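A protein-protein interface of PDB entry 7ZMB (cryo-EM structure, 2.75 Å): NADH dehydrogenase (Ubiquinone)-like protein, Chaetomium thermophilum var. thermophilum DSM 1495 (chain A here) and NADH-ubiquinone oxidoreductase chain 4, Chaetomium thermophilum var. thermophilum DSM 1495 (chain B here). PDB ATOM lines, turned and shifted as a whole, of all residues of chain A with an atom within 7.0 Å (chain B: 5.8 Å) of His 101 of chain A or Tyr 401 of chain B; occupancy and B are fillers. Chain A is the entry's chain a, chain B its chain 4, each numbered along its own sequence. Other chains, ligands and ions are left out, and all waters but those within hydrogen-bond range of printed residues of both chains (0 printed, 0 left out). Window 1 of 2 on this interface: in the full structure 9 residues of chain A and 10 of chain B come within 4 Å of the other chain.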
ATOM      1  N   TYR A  67     -11.765 -19.882   9.810  1.00  0.00           N
ATOM      2  CA  TYR A  67     -10.582 -19.787  10.651  1.00  0.00           C
ATOM      3  C   TYR A  67      -9.612 -20.920  10.329  1.00  0.00           C
ATOM      4  O   TYR A  67      -9.987 -22.093  10.309  1.00  0.00           O
ATOM      5  CB  TYR A  67     -10.995 -19.830  12.123  1.00  0.00           C
ATOM      6  CG  TYR A  67      -9.854 -19.802  13.105  1.00  0.00           C
ATOM      7  CD1 TYR A  67      -9.324 -18.599  13.552  1.00  0.00           C
ATOM      8  CD2 TYR A  67      -9.317 -20.975  13.599  1.00  0.00           C
ATOM      9  CE1 TYR A  67      -8.281 -18.573  14.462  1.00  0.00           C
ATOM     10  CE2 TYR A  67      -8.278 -20.961  14.497  1.00  0.00           C
ATOM     11  CZ  TYR A  67      -7.761 -19.761  14.929  1.00  0.00           C
ATOM     12  OH  TYR A  67      -6.724 -19.758  15.835  1.00  0.00           O
ATOM     13  N   ARG A  72      -4.072 -30.069  15.811  1.00  0.00           N
ATOM     14  CA  ARG A  72      -4.467 -30.036  17.217  1.00  0.00           C
ATOM     15  C   ARG A  72      -3.534 -30.939  18.012  1.00  0.00           C
ATOM     16  O   ARG A  72      -3.762 -32.142  18.151  1.00  0.00           O
ATOM     17  CB  ARG A  72      -5.921 -30.461  17.373  1.00  0.00           C
ATOM     18  CG  ARG A  72      -6.448 -30.305  18.778  1.00  0.00           C
ATOM     19  CD  ARG A  72      -7.953 -30.157  18.804  1.00  0.00           C
ATOM     20  NE  ARG A  72      -8.440 -29.783  20.130  1.00  0.00           N
ATOM     21  CZ  ARG A  72      -8.450 -30.593  21.185  1.00  0.00           C
ATOM     22  NH1 ARG A  72      -8.912 -30.155  22.349  1.00  0.00           N
ATOM     23  NH2 ARG A  72      -8.009 -31.839  21.080  1.00  0.00           N
ATOM     24  N   ARG A  75       1.037 -28.911  23.607  1.00  0.00           N
ATOM     25  CA  ARG A  75       2.402 -28.411  23.648  1.00  0.00           C
ATOM     26  C   ARG A  75       3.313 -29.285  24.488  1.00  0.00           C
ATOM     27  O   ARG A  75       4.510 -28.997  24.577  1.00  0.00           O
ATOM     28  CB  ARG A  75       2.441 -26.980  24.177  1.00  0.00           C
ATOM     29  CG  ARG A  75       1.541 -26.056  23.429  1.00  0.00           C
ATOM     30  CD  ARG A  75       1.932 -24.611  23.631  1.00  0.00           C
ATOM     31  NE  ARG A  75       0.820 -23.710  23.353  1.00  0.00           N
ATOM     32  CZ  ARG A  75       0.270 -23.549  22.155  1.00  0.00           C
ATOM     33  NH1 ARG A  75      -0.739 -22.710  22.002  1.00  0.00           N
ATOM     34  NH2 ARG A  75       0.730 -24.216  21.105  1.00  0.00           N
ATOM     35  N   GLU A  89       5.865 -21.773  27.922  1.00  0.00           N
ATOM     36  CA  GLU A  89       4.745 -22.279  27.146  1.00  0.00           C
ATOM     37  C   GLU A  89       5.177 -23.107  25.944  1.00  0.00           C
ATOM     38  O   GLU A  89       4.366 -23.876  25.422  1.00  0.00           O
ATOM     39  CB  GLU A  89       3.872 -21.097  26.686  1.00  0.00           C
ATOM     40  CG  GLU A  89       2.623 -21.447  25.895  1.00  0.00           C
ATOM     41  CD  GLU A  89       1.609 -22.227  26.705  1.00  0.00           C
ATOM     42  OE1 GLU A  89       1.605 -22.099  27.946  1.00  0.00           O
ATOM     43  OE2 GLU A  89       0.805 -22.960  26.093  1.00  0.00           O
ATOM     44  N   ARG A  91       6.120 -21.837  22.944  1.00  0.00           N
ATOM     45  CA  ARG A  91       5.374 -21.226  21.860  1.00  0.00           C
ATOM     46  C   ARG A  91       6.177 -20.077  21.274  1.00  0.00           C
ATOM     47  O   ARG A  91       6.817 -19.317  22.007  1.00  0.00           O
ATOM     48  CB  ARG A  91       4.008 -20.730  22.349  1.00  0.00           C
ATOM     49  CG  ARG A  91       3.007 -20.493  21.244  1.00  0.00           C
ATOM     50  CD  ARG A  91       1.804 -19.710  21.733  1.00  0.00           C
ATOM     51  NE  ARG A  91       1.137 -19.038  20.628  1.00  0.00           N
ATOM     52  CZ  ARG A  91       1.270 -17.747  20.350  1.00  0.00           C
ATOM     53  NH1 ARG A  91       2.033 -16.974  21.109  1.00  0.00           N
ATOM     54  NH2 ARG A  91       0.631 -17.224  19.319  1.00  0.00           N
ATOM     55  N   GLU A  95       3.127 -17.376  16.817  1.00  0.00           N
ATOM     56  CA  GLU A  95       2.810 -18.700  16.309  1.00  0.00           C
ATOM     57  C   GLU A  95       1.299 -18.862  16.169  1.00  0.00           C
ATOM     58  O   GLU A  95       0.546 -18.467  17.068  1.00  0.00           O
ATOM     59  CB  GLU A  95       3.374 -19.770  17.244  1.00  0.00           C
ATOM     60  CG  GLU A  95       3.299 -21.181  16.698  1.00  0.00           C
ATOM     61  CD  GLU A  95       4.180 -22.149  17.462  1.00  0.00           C
ATOM     62  OE1 GLU A  95       4.881 -21.707  18.398  1.00  0.00           O
ATOM     63  OE2 GLU A  95       4.171 -23.353  17.129  1.00  0.00           O
ATOM     64  N   PRO A  96       0.820 -19.414  15.058  1.00  0.00           N
ATOM     65  CA  PRO A  96      -0.615 -19.671  14.923  1.00  0.00           C
ATOM     66  C   PRO A  96      -1.111 -20.586  16.030  1.00  0.00           C
ATOM     67  O   PRO A  96      -0.345 -21.299  16.678  1.00  0.00           O
ATOM     68  CB  PRO A  96      -0.736 -20.335  13.545  1.00  0.00           C
ATOM     69  CG  PRO A  96       0.655 -20.736  13.175  1.00  0.00           C
ATOM     70  CD  PRO A  96       1.557 -19.752  13.835  1.00  0.00           C
ATOM     71  N   VAL A  97      -2.416 -20.546  16.255  1.00  0.00           N
ATOM     72  CA  VAL A  97      -3.016 -21.133  17.445  1.00  0.00           C
ATOM     73  C   VAL A  97      -4.287 -21.868  17.052  1.00  0.00           C
ATOM     74  O   VAL A  97      -5.042 -21.413  16.185  1.00  0.00           O
ATOM     75  CB  VAL A  97      -3.310 -20.050  18.505  1.00  0.00           C
ATOM     76  CG1 VAL A  97      -2.027 -19.570  19.151  1.00  0.00           C
ATOM     77  CG2 VAL A  97      -4.026 -18.888  17.880  1.00  0.00           C
ATOM     78  N   HIS A  98      -4.516 -23.015  17.682  1.00  0.00           N
ATOM     79  CA  HIS A  98      -5.761 -23.746  17.525  1.00  0.00           C
ATOM     80  C   HIS A  98      -6.895 -23.033  18.258  1.00  0.00           C
ATOM     81  O   HIS A  98      -6.677 -22.289  19.214  1.00  0.00           O
ATOM     82  CB  HIS A  98      -5.605 -25.167  18.057  1.00  0.00           C
ATOM     83  CG  HIS A  98      -6.635 -26.124  17.552  1.00  0.00           C
ATOM     84  ND1 HIS A  98      -7.927 -26.144  18.023  1.00  0.00           N
ATOM     85  CD2 HIS A  98      -6.560 -27.103  16.621  1.00  0.00           C
ATOM     86  CE1 HIS A  98      -8.609 -27.085  17.398  1.00  0.00           C
ATOM     87  NE2 HIS A  98      -7.801 -27.682  16.541  1.00  0.00           N
ATOM     88  N   GLU A  99      -8.127 -23.276  17.807  1.00  0.00           N
ATOM     89  CA  GLU A  99      -9.269 -22.742  18.541  1.00  0.00           C
ATOM     90  C   GLU A  99      -9.455 -23.405  19.898  1.00  0.00           C
ATOM     91  O   GLU A  99     -10.250 -22.916  20.706  1.00  0.00           O
ATOM     92  CB  GLU A  99     -10.546 -22.864  17.715  1.00  0.00           C
ATOM     93  CG  GLU A  99     -11.188 -24.213  17.710  1.00  0.00           C
ATOM     94  CD  GLU A  99     -12.063 -24.407  16.486  1.00  0.00           C
ATOM     95  OE1 GLU A  99     -11.567 -24.958  15.481  1.00  0.00           O
ATOM     96  OE2 GLU A  99     -13.239 -23.994  16.524  1.00  0.00           O
ATOM     97  N   ASP A 100      -8.746 -24.500  20.162  1.00  0.00           N
ATOM     98  CA  ASP A 100      -8.634 -25.073  21.493  1.00  0.00           C
ATOM     99  C   ASP A 100      -7.331 -24.670  22.170  1.00  0.00           C
ATOM    100  O   ASP A 100      -6.785 -25.436  22.970  1.00  0.00           O
ATOM    101  CB  ASP A 100      -8.757 -26.593  21.424  1.00  0.00           C
ATOM    102  CG  ASP A 100     -10.180 -27.049  21.187  1.00  0.00           C
ATOM    103  OD1 ASP A 100     -11.057 -26.187  20.985  1.00  0.00           O
ATOM    104  OD2 ASP A 100     -10.428 -28.270  21.208  1.00  0.00           O
ATOM    105  N   HIS A 101      -6.815 -23.487  21.841  1.00  0.00           N
ATOM    106  CA  HIS A 101      -5.535 -23.011  22.439  1.00  0.00           C
ATOM    107  C   HIS A 101      -5.627 -23.087  23.958  1.00  0.00           C
ATOM    108  O   HIS A 101      -4.613 -23.444  24.580  1.00  0.00           O
ATOM    109  CB  HIS A 101      -5.222 -21.585  21.965  1.00  0.00           C
ATOM    110  CG  HIS A 101      -4.141 -20.879  22.714  1.00  0.00           C
ATOM    111  ND1 HIS A 101      -2.887 -20.672  22.179  1.00  0.00           N
ATOM    112  CD2 HIS A 101      -4.122 -20.306  23.937  1.00  0.00           C
ATOM    113  CE1 HIS A 101      -2.140 -20.020  23.046  1.00  0.00           C
ATOM    114  NE2 HIS A 101      -2.874 -19.786  24.134  1.00  0.00           N
ATOM    115  N   ASP A 102      -6.802 -22.790  24.524  1.00  0.00           N
ATOM    116  CA  ASP A 102      -6.926 -22.721  25.973  1.00  0.00           C
ATOM    117  C   ASP A 102      -6.653 -24.062  26.641  1.00  0.00           C
ATOM    118  O   ASP A 102      -6.163 -24.091  27.774  1.00  0.00           O
ATOM    119  CB  ASP A 102      -8.312 -22.197  26.368  1.00  0.00           C
ATOM    120  CG  ASP A 102      -9.450 -22.932  25.671  1.00  0.00           C
ATOM    121  OD1 ASP A 102      -9.217 -23.537  24.606  1.00  0.00           O
ATOM    122  OD2 ASP A 102     -10.580 -22.907  26.199  1.00  0.00           O
ATOM    123  N   ILE A 103      -6.957 -25.174  25.979  1.00  0.00           N
ATOM    124  CA  ILE A 103      -6.774 -26.489  26.582  1.00  0.00           C
ATOM    125  C   ILE A 103      -5.750 -27.323  25.820  1.00  0.00           C
ATOM    126  O   ILE A 103      -5.736 -28.539  25.933  1.00  0.00           O
ATOM    127  CB  ILE A 103      -8.111 -27.242  26.715  1.00  0.00           C
ATOM    128  CG1 ILE A 103      -8.728 -27.509  25.339  1.00  0.00           C
ATOM    129  CG2 ILE A 103      -9.064 -26.473  27.597  1.00  0.00           C
ATOM    130  CD1 ILE A 103      -9.686 -28.677  25.306  1.00  0.00           C
ATOM    131  N   LEU A 104      -4.886 -26.675  25.041  1.00  0.00           N
ATOM    132  CA  LEU A 104      -3.804 -27.351  24.340  1.00  0.00           C
ATOM    133  C   LEU A 104      -2.432 -26.864  24.766  1.00  0.00           C
ATOM    134  O   LEU A 104      -1.447 -27.157  24.078  1.00  0.00           O
ATOM    135  CB  LEU A 104      -3.950 -27.172  22.827  1.00  0.00           C
ATOM    136  CG  LEU A 104      -5.011 -28.000  22.124  1.00  0.00           C
ATOM    137  CD1 LEU A 104      -5.050 -27.635  20.660  1.00  0.00           C
ATOM    138  CD2 LEU A 104      -4.715 -29.471  22.297  1.00  0.00           C
ATOM    139  N   GLY A 105      -2.337 -26.127  25.864  1.00  0.00           N
ATOM    140  CA  GLY A 105      -1.085 -25.546  26.289  1.00  0.00           C
ATOM    141  C   GLY A 105      -0.389 -26.384  27.338  1.00  0.00           C
ATOM    142  O   GLY A 105      -0.761 -27.523  27.625  1.00  0.00           O
ATOM    143  N   MET A 106       0.651 -25.792  27.928  1.00  0.00           N
ATOM    144  CA  MET A 106       1.432 -26.517  28.926  1.00  0.00           C
ATOM    145  C   MET A 106       0.639 -26.745  30.210  1.00  0.00           C
ATOM    146  O   MET A 106       0.732 -27.817  30.816  1.00  0.00           O
ATOM    147  CB  MET A 106       2.735 -25.778  29.215  1.00  0.00           C
ATOM    148  CG  MET A 106       3.692 -25.769  28.048  1.00  0.00           C
ATOM    149  SD  MET A 106       4.117 -27.411  27.462  1.00  0.00           S
ATOM    150  CE  MET A 106       5.164 -27.988  28.797  1.00  0.00           C
ATOM    151  N   SER A 108      -2.301 -27.731  30.867  1.00  0.00           N
ATOM    152  CA  SER A 108      -3.442 -28.545  30.479  1.00  0.00           C
ATOM    153  C   SER A 108      -3.253 -29.913  31.106  1.00  0.00           C
ATOM    154  O   SER A 108      -2.153 -30.233  31.570  1.00  0.00           O
ATOM    155  CB  SER A 108      -3.562 -28.665  28.952  1.00  0.00           C
ATOM    156  OG  SER A 108      -4.151 -27.515  28.383  1.00  0.00           O
ATOM    157  N   ARG B 335     -14.634 -23.449  29.834  1.00  0.00           N
ATOM    158  CA  ARG B 335     -13.965 -23.228  28.556  1.00  0.00           C
ATOM    159  C   ARG B 335     -13.946 -21.763  28.126  1.00  0.00           C
ATOM    160  O   ARG B 335     -13.579 -21.472  26.986  1.00  0.00           O
ATOM    161  CB  ARG B 335     -14.632 -24.063  27.461  1.00  0.00           C
ATOM    162  CG  ARG B 335     -14.326 -25.542  27.505  1.00  0.00           C
ATOM    163  CD  ARG B 335     -12.839 -25.834  27.356  1.00  0.00           C
ATOM    164  NE  ARG B 335     -12.288 -25.384  26.085  1.00  0.00           N
ATOM    165  CZ  ARG B 335     -12.290 -26.100  24.968  1.00  0.00           C
ATOM    166  NH1 ARG B 335     -12.830 -27.312  24.943  1.00  0.00           N
ATOM    167  NH2 ARG B 335     -11.753 -25.603  23.867  1.00  0.00           N
ATOM    168  N   VAL B 337     -12.846 -17.960  27.580  1.00  0.00           N
ATOM    169  CA  VAL B 337     -11.564 -17.290  27.395  1.00  0.00           C
ATOM    170  C   VAL B 337     -11.600 -15.849  27.887  1.00  0.00           C
ATOM    171  O   VAL B 337     -10.628 -15.362  28.460  1.00  0.00           O
ATOM    172  CB  VAL B 337     -11.149 -17.362  25.911  1.00  0.00           C
ATOM    173  CG1 VAL B 337      -9.878 -16.583  25.676  1.00  0.00           C
ATOM    174  CG2 VAL B 337     -10.978 -18.804  25.486  1.00  0.00           C
ATOM    175  N   LEU B 399      -8.658 -11.265  27.450  1.00  0.00           N
ATOM    176  CA  LEU B 399      -8.337 -12.614  27.014  1.00  0.00           C
ATOM    177  C   LEU B 399      -7.392 -13.257  28.016  1.00  0.00           C
ATOM    178  O   LEU B 399      -6.300 -12.740  28.266  1.00  0.00           O
ATOM    179  CB  LEU B 399      -7.710 -12.581  25.625  1.00  0.00           C
ATOM    180  CG  LEU B 399      -8.611 -12.123  24.485  1.00  0.00           C
ATOM    181  CD1 LEU B 399      -8.086 -12.649  23.164  1.00  0.00           C
ATOM    182  CD2 LEU B 399     -10.041 -12.572  24.725  1.00  0.00           C
ATOM    183  N   ILE B 400      -7.808 -14.392  28.576  1.00  0.00           N
ATOM    184  CA  ILE B 400      -7.011 -15.080  29.581  1.00  0.00           C
ATOM    185  C   ILE B 400      -5.690 -15.591  29.014  1.00  0.00           C
ATOM    186  O   ILE B 400      -4.772 -15.899  29.779  1.00  0.00           O
ATOM    187  CB  ILE B 400      -7.841 -16.222  30.201  1.00  0.00           C
ATOM    188  CG1 ILE B 400      -7.271 -16.620  31.564  1.00  0.00           C
ATOM    189  CG2 ILE B 400      -7.919 -17.405  29.253  1.00  0.00           C
ATOM    190  CD1 ILE B 400      -8.203 -17.430  32.403  1.00  0.00           C
ATOM    191  N   TYR B 401      -5.567 -15.678  27.685  1.00  0.00           N
ATOM    192  CA  TYR B 401      -4.305 -16.051  27.053  1.00  0.00           C
ATOM    193  C   TYR B 401      -3.163 -15.141  27.457  1.00  0.00           C
ATOM    194  O   TYR B 401      -2.009 -15.581  27.478  1.00  0.00           O
ATOM    195  CB  TYR B 401      -4.416 -15.993  25.533  1.00  0.00           C
ATOM    196  CG  TYR B 401      -5.555 -16.758  24.921  1.00  0.00           C
ATOM    197  CD1 TYR B 401      -5.943 -17.986  25.423  1.00  0.00           C
ATOM    198  CD2 TYR B 401      -6.227 -16.257  23.817  1.00  0.00           C
ATOM    199  CE1 TYR B 401      -6.980 -18.690  24.849  1.00  0.00           C
ATOM    200  CE2 TYR B 401      -7.265 -16.957  23.237  1.00  0.00           C
ATOM    201  CZ  TYR B 401      -7.631 -18.173  23.755  1.00  0.00           C
ATOM    202  OH  TYR B 401      -8.664 -18.875  23.188  1.00  0.00           O
ATOM    203  N   PHE B 402      -3.452 -13.883  27.754  1.00  0.00           N
ATOM    204  CA  PHE B 402      -2.435 -12.880  27.997  1.00  0.00           C
ATOM    205  C   PHE B 402      -2.037 -12.774  29.458  1.00  0.00           C
ATOM    206  O   PHE B 402      -1.190 -11.945  29.790  1.00  0.00           O
ATOM    207  CB  PHE B 402      -2.927 -11.518  27.523  1.00  0.00           C
ATOM    208  CG  PHE B 402      -2.894 -11.339  26.041  1.00  0.00           C
ATOM    209  CD1 PHE B 402      -1.696 -11.266  25.371  1.00  0.00           C
ATOM    210  CD2 PHE B 402      -4.065 -11.201  25.328  1.00  0.00           C
ATOM    211  CE1 PHE B 402      -1.663 -11.080  24.011  1.00  0.00           C
ATOM    212  CE2 PHE B 402      -4.039 -11.020  23.969  1.00  0.00           C
ATOM    213  CZ  PHE B 402      -2.837 -10.957  23.307  1.00  0.00           C
ATOM    214  N   PHE B 403      -2.647 -13.559  30.338  1.00  0.00           N
ATOM    215  CA  PHE B 403      -2.417 -13.453  31.769  1.00  0.00           C
ATOM    216  C   PHE B 403      -1.859 -14.761  32.294  1.00  0.00           C
ATOM    217  O   PHE B 403      -2.308 -15.842  31.909  1.00  0.00           O
ATOM    218  CB  PHE B 403      -3.690 -13.096  32.523  1.00  0.00           C
ATOM    219  CG  PHE B 403      -4.328 -11.826  32.065  1.00  0.00           C
ATOM    220  CD1 PHE B 403      -3.986 -10.623  32.642  1.00  0.00           C
ATOM    221  CD2 PHE B 403      -5.269 -11.836  31.056  1.00  0.00           C
ATOM    222  CE1 PHE B 403      -4.574  -9.456  32.218  1.00  0.00           C
ATOM    223  CE2 PHE B 403      -5.854 -10.674  30.627  1.00  0.00           C
ATOM    224  CZ  PHE B 403      -5.512  -9.483  31.205  1.00  0.00           C
ATOM    225  N   SER B 479       3.161 -13.356  32.587  1.00  0.00           N
ATOM    226  CA  SER B 479       2.901 -13.456  31.165  1.00  0.00           C
ATOM    227  C   SER B 479       3.922 -12.617  30.404  1.00  0.00           C
ATOM    228  O   SER B 479       4.173 -11.460  30.744  1.00  0.00           O
ATOM    229  CB  SER B 479       1.477 -13.003  30.862  1.00  0.00           C
ATOM    230  OG  SER B 479       1.205 -13.047  29.480  1.00  0.00           O
ATOM    231  N   TYR B 481       3.692 -11.468  27.466  1.00  0.00           N
ATOM    232  CA  TYR B 481       3.115 -10.417  26.648  1.00  0.00           C
ATOM    233  C   TYR B 481       3.109  -9.062  27.351  1.00  0.00           C
ATOM    234  O   TYR B 481       2.782  -8.055  26.717  1.00  0.00           O
ATOM    235  CB  TYR B 481       1.700 -10.794  26.226  1.00  0.00           C
ATOM    236  CG  TYR B 481       1.559 -12.179  25.642  1.00  0.00           C
ATOM    237  CD1 TYR B 481       1.364 -13.281  26.455  1.00  0.00           C
ATOM    238  CD2 TYR B 481       1.589 -12.380  24.271  1.00  0.00           C
ATOM    239  CE1 TYR B 481       1.226 -14.540  25.926  1.00  0.00           C
ATOM    240  CE2 TYR B 481       1.444 -13.642  23.732  1.00  0.00           C
ATOM    241  CZ  TYR B 481       1.265 -14.717  24.568  1.00  0.00           C
ATOM    242  OH  TYR B 481       1.123 -15.975  24.043  1.00  0.00           O
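Among the printed residues, pairs that only touch across the chains: His 101 of chain A with Tyr 401 of chain B (3.3 Å) and Ile 103 of chain A with Arg 335 of chain B (3.4 Å).
Of chain B, only Tyr 401 comes within 4 Å of His 101 of chain A. Of the printed residues of chain A, Tyr 401 of chain B touches His 101 (3.3 Å). Of the printed residues of chain A, Arg 335 of chain B touches Asp 100, Asp 102 and Ile 103. Of the printed residues of chain A, Tyr 481 of chain B touches Arg 91 (3.2 Å). Tyr 67 of chain A touches none of the printed residues of chain B. The nearest residue of chain B that does not touch His 101 of chain A is Tyr 481 of chain B (5.3 Å).
OH of Tyr 481 of chain B is in hydrogen-bond range of NH1 of Arg 91 of chain A, 3.2 Å away. The guanidinium group (NH2) of Arg 335 of chain B lies within salt-bridge range of the side-chain carboxylate (OD1) of Asp 100 of chain A, at 3.0 Å. The guanidinium group (NE) of Arg 335 of chain B lies within salt-bridge range of the side-chain carboxylate (OD2) of Asp 102 of chain A (3.0 Å).
Of the 18 printed residues of chain A, 5 touch a printed residue of chain B. Hydrophobic or aromatic side chains of chain A within 4 Å of the printed part of chain B: His 101 and Ile 103. Among the printed residues, 5 pairs touch across the chains.
The side-chain carboxylate (OD2) of Asp 100 of chain A is in salt-bridge range of the guanidinium group (NH1) of Arg 72 of chain A (2.7 Å). A ring nitrogen (ND1) of His 101 of chain A lies within hydrogen-bond range of the guanidinium group (NH1) of Arg 75 of chain A. The guanidinium group (NH2) of Arg 91 of chain A is in hydrogen-bond range of the backbone carbonyl oxygen (O) of Glu 95 of chain A (2.6 Å). ND1 of His 98 of chain A sits at hydrogen-bond distance from N of Asp 100 of chain A. O of Ile 103 of chain A lies close to OG of Ser 108 of chain A, at 3.1 Å.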
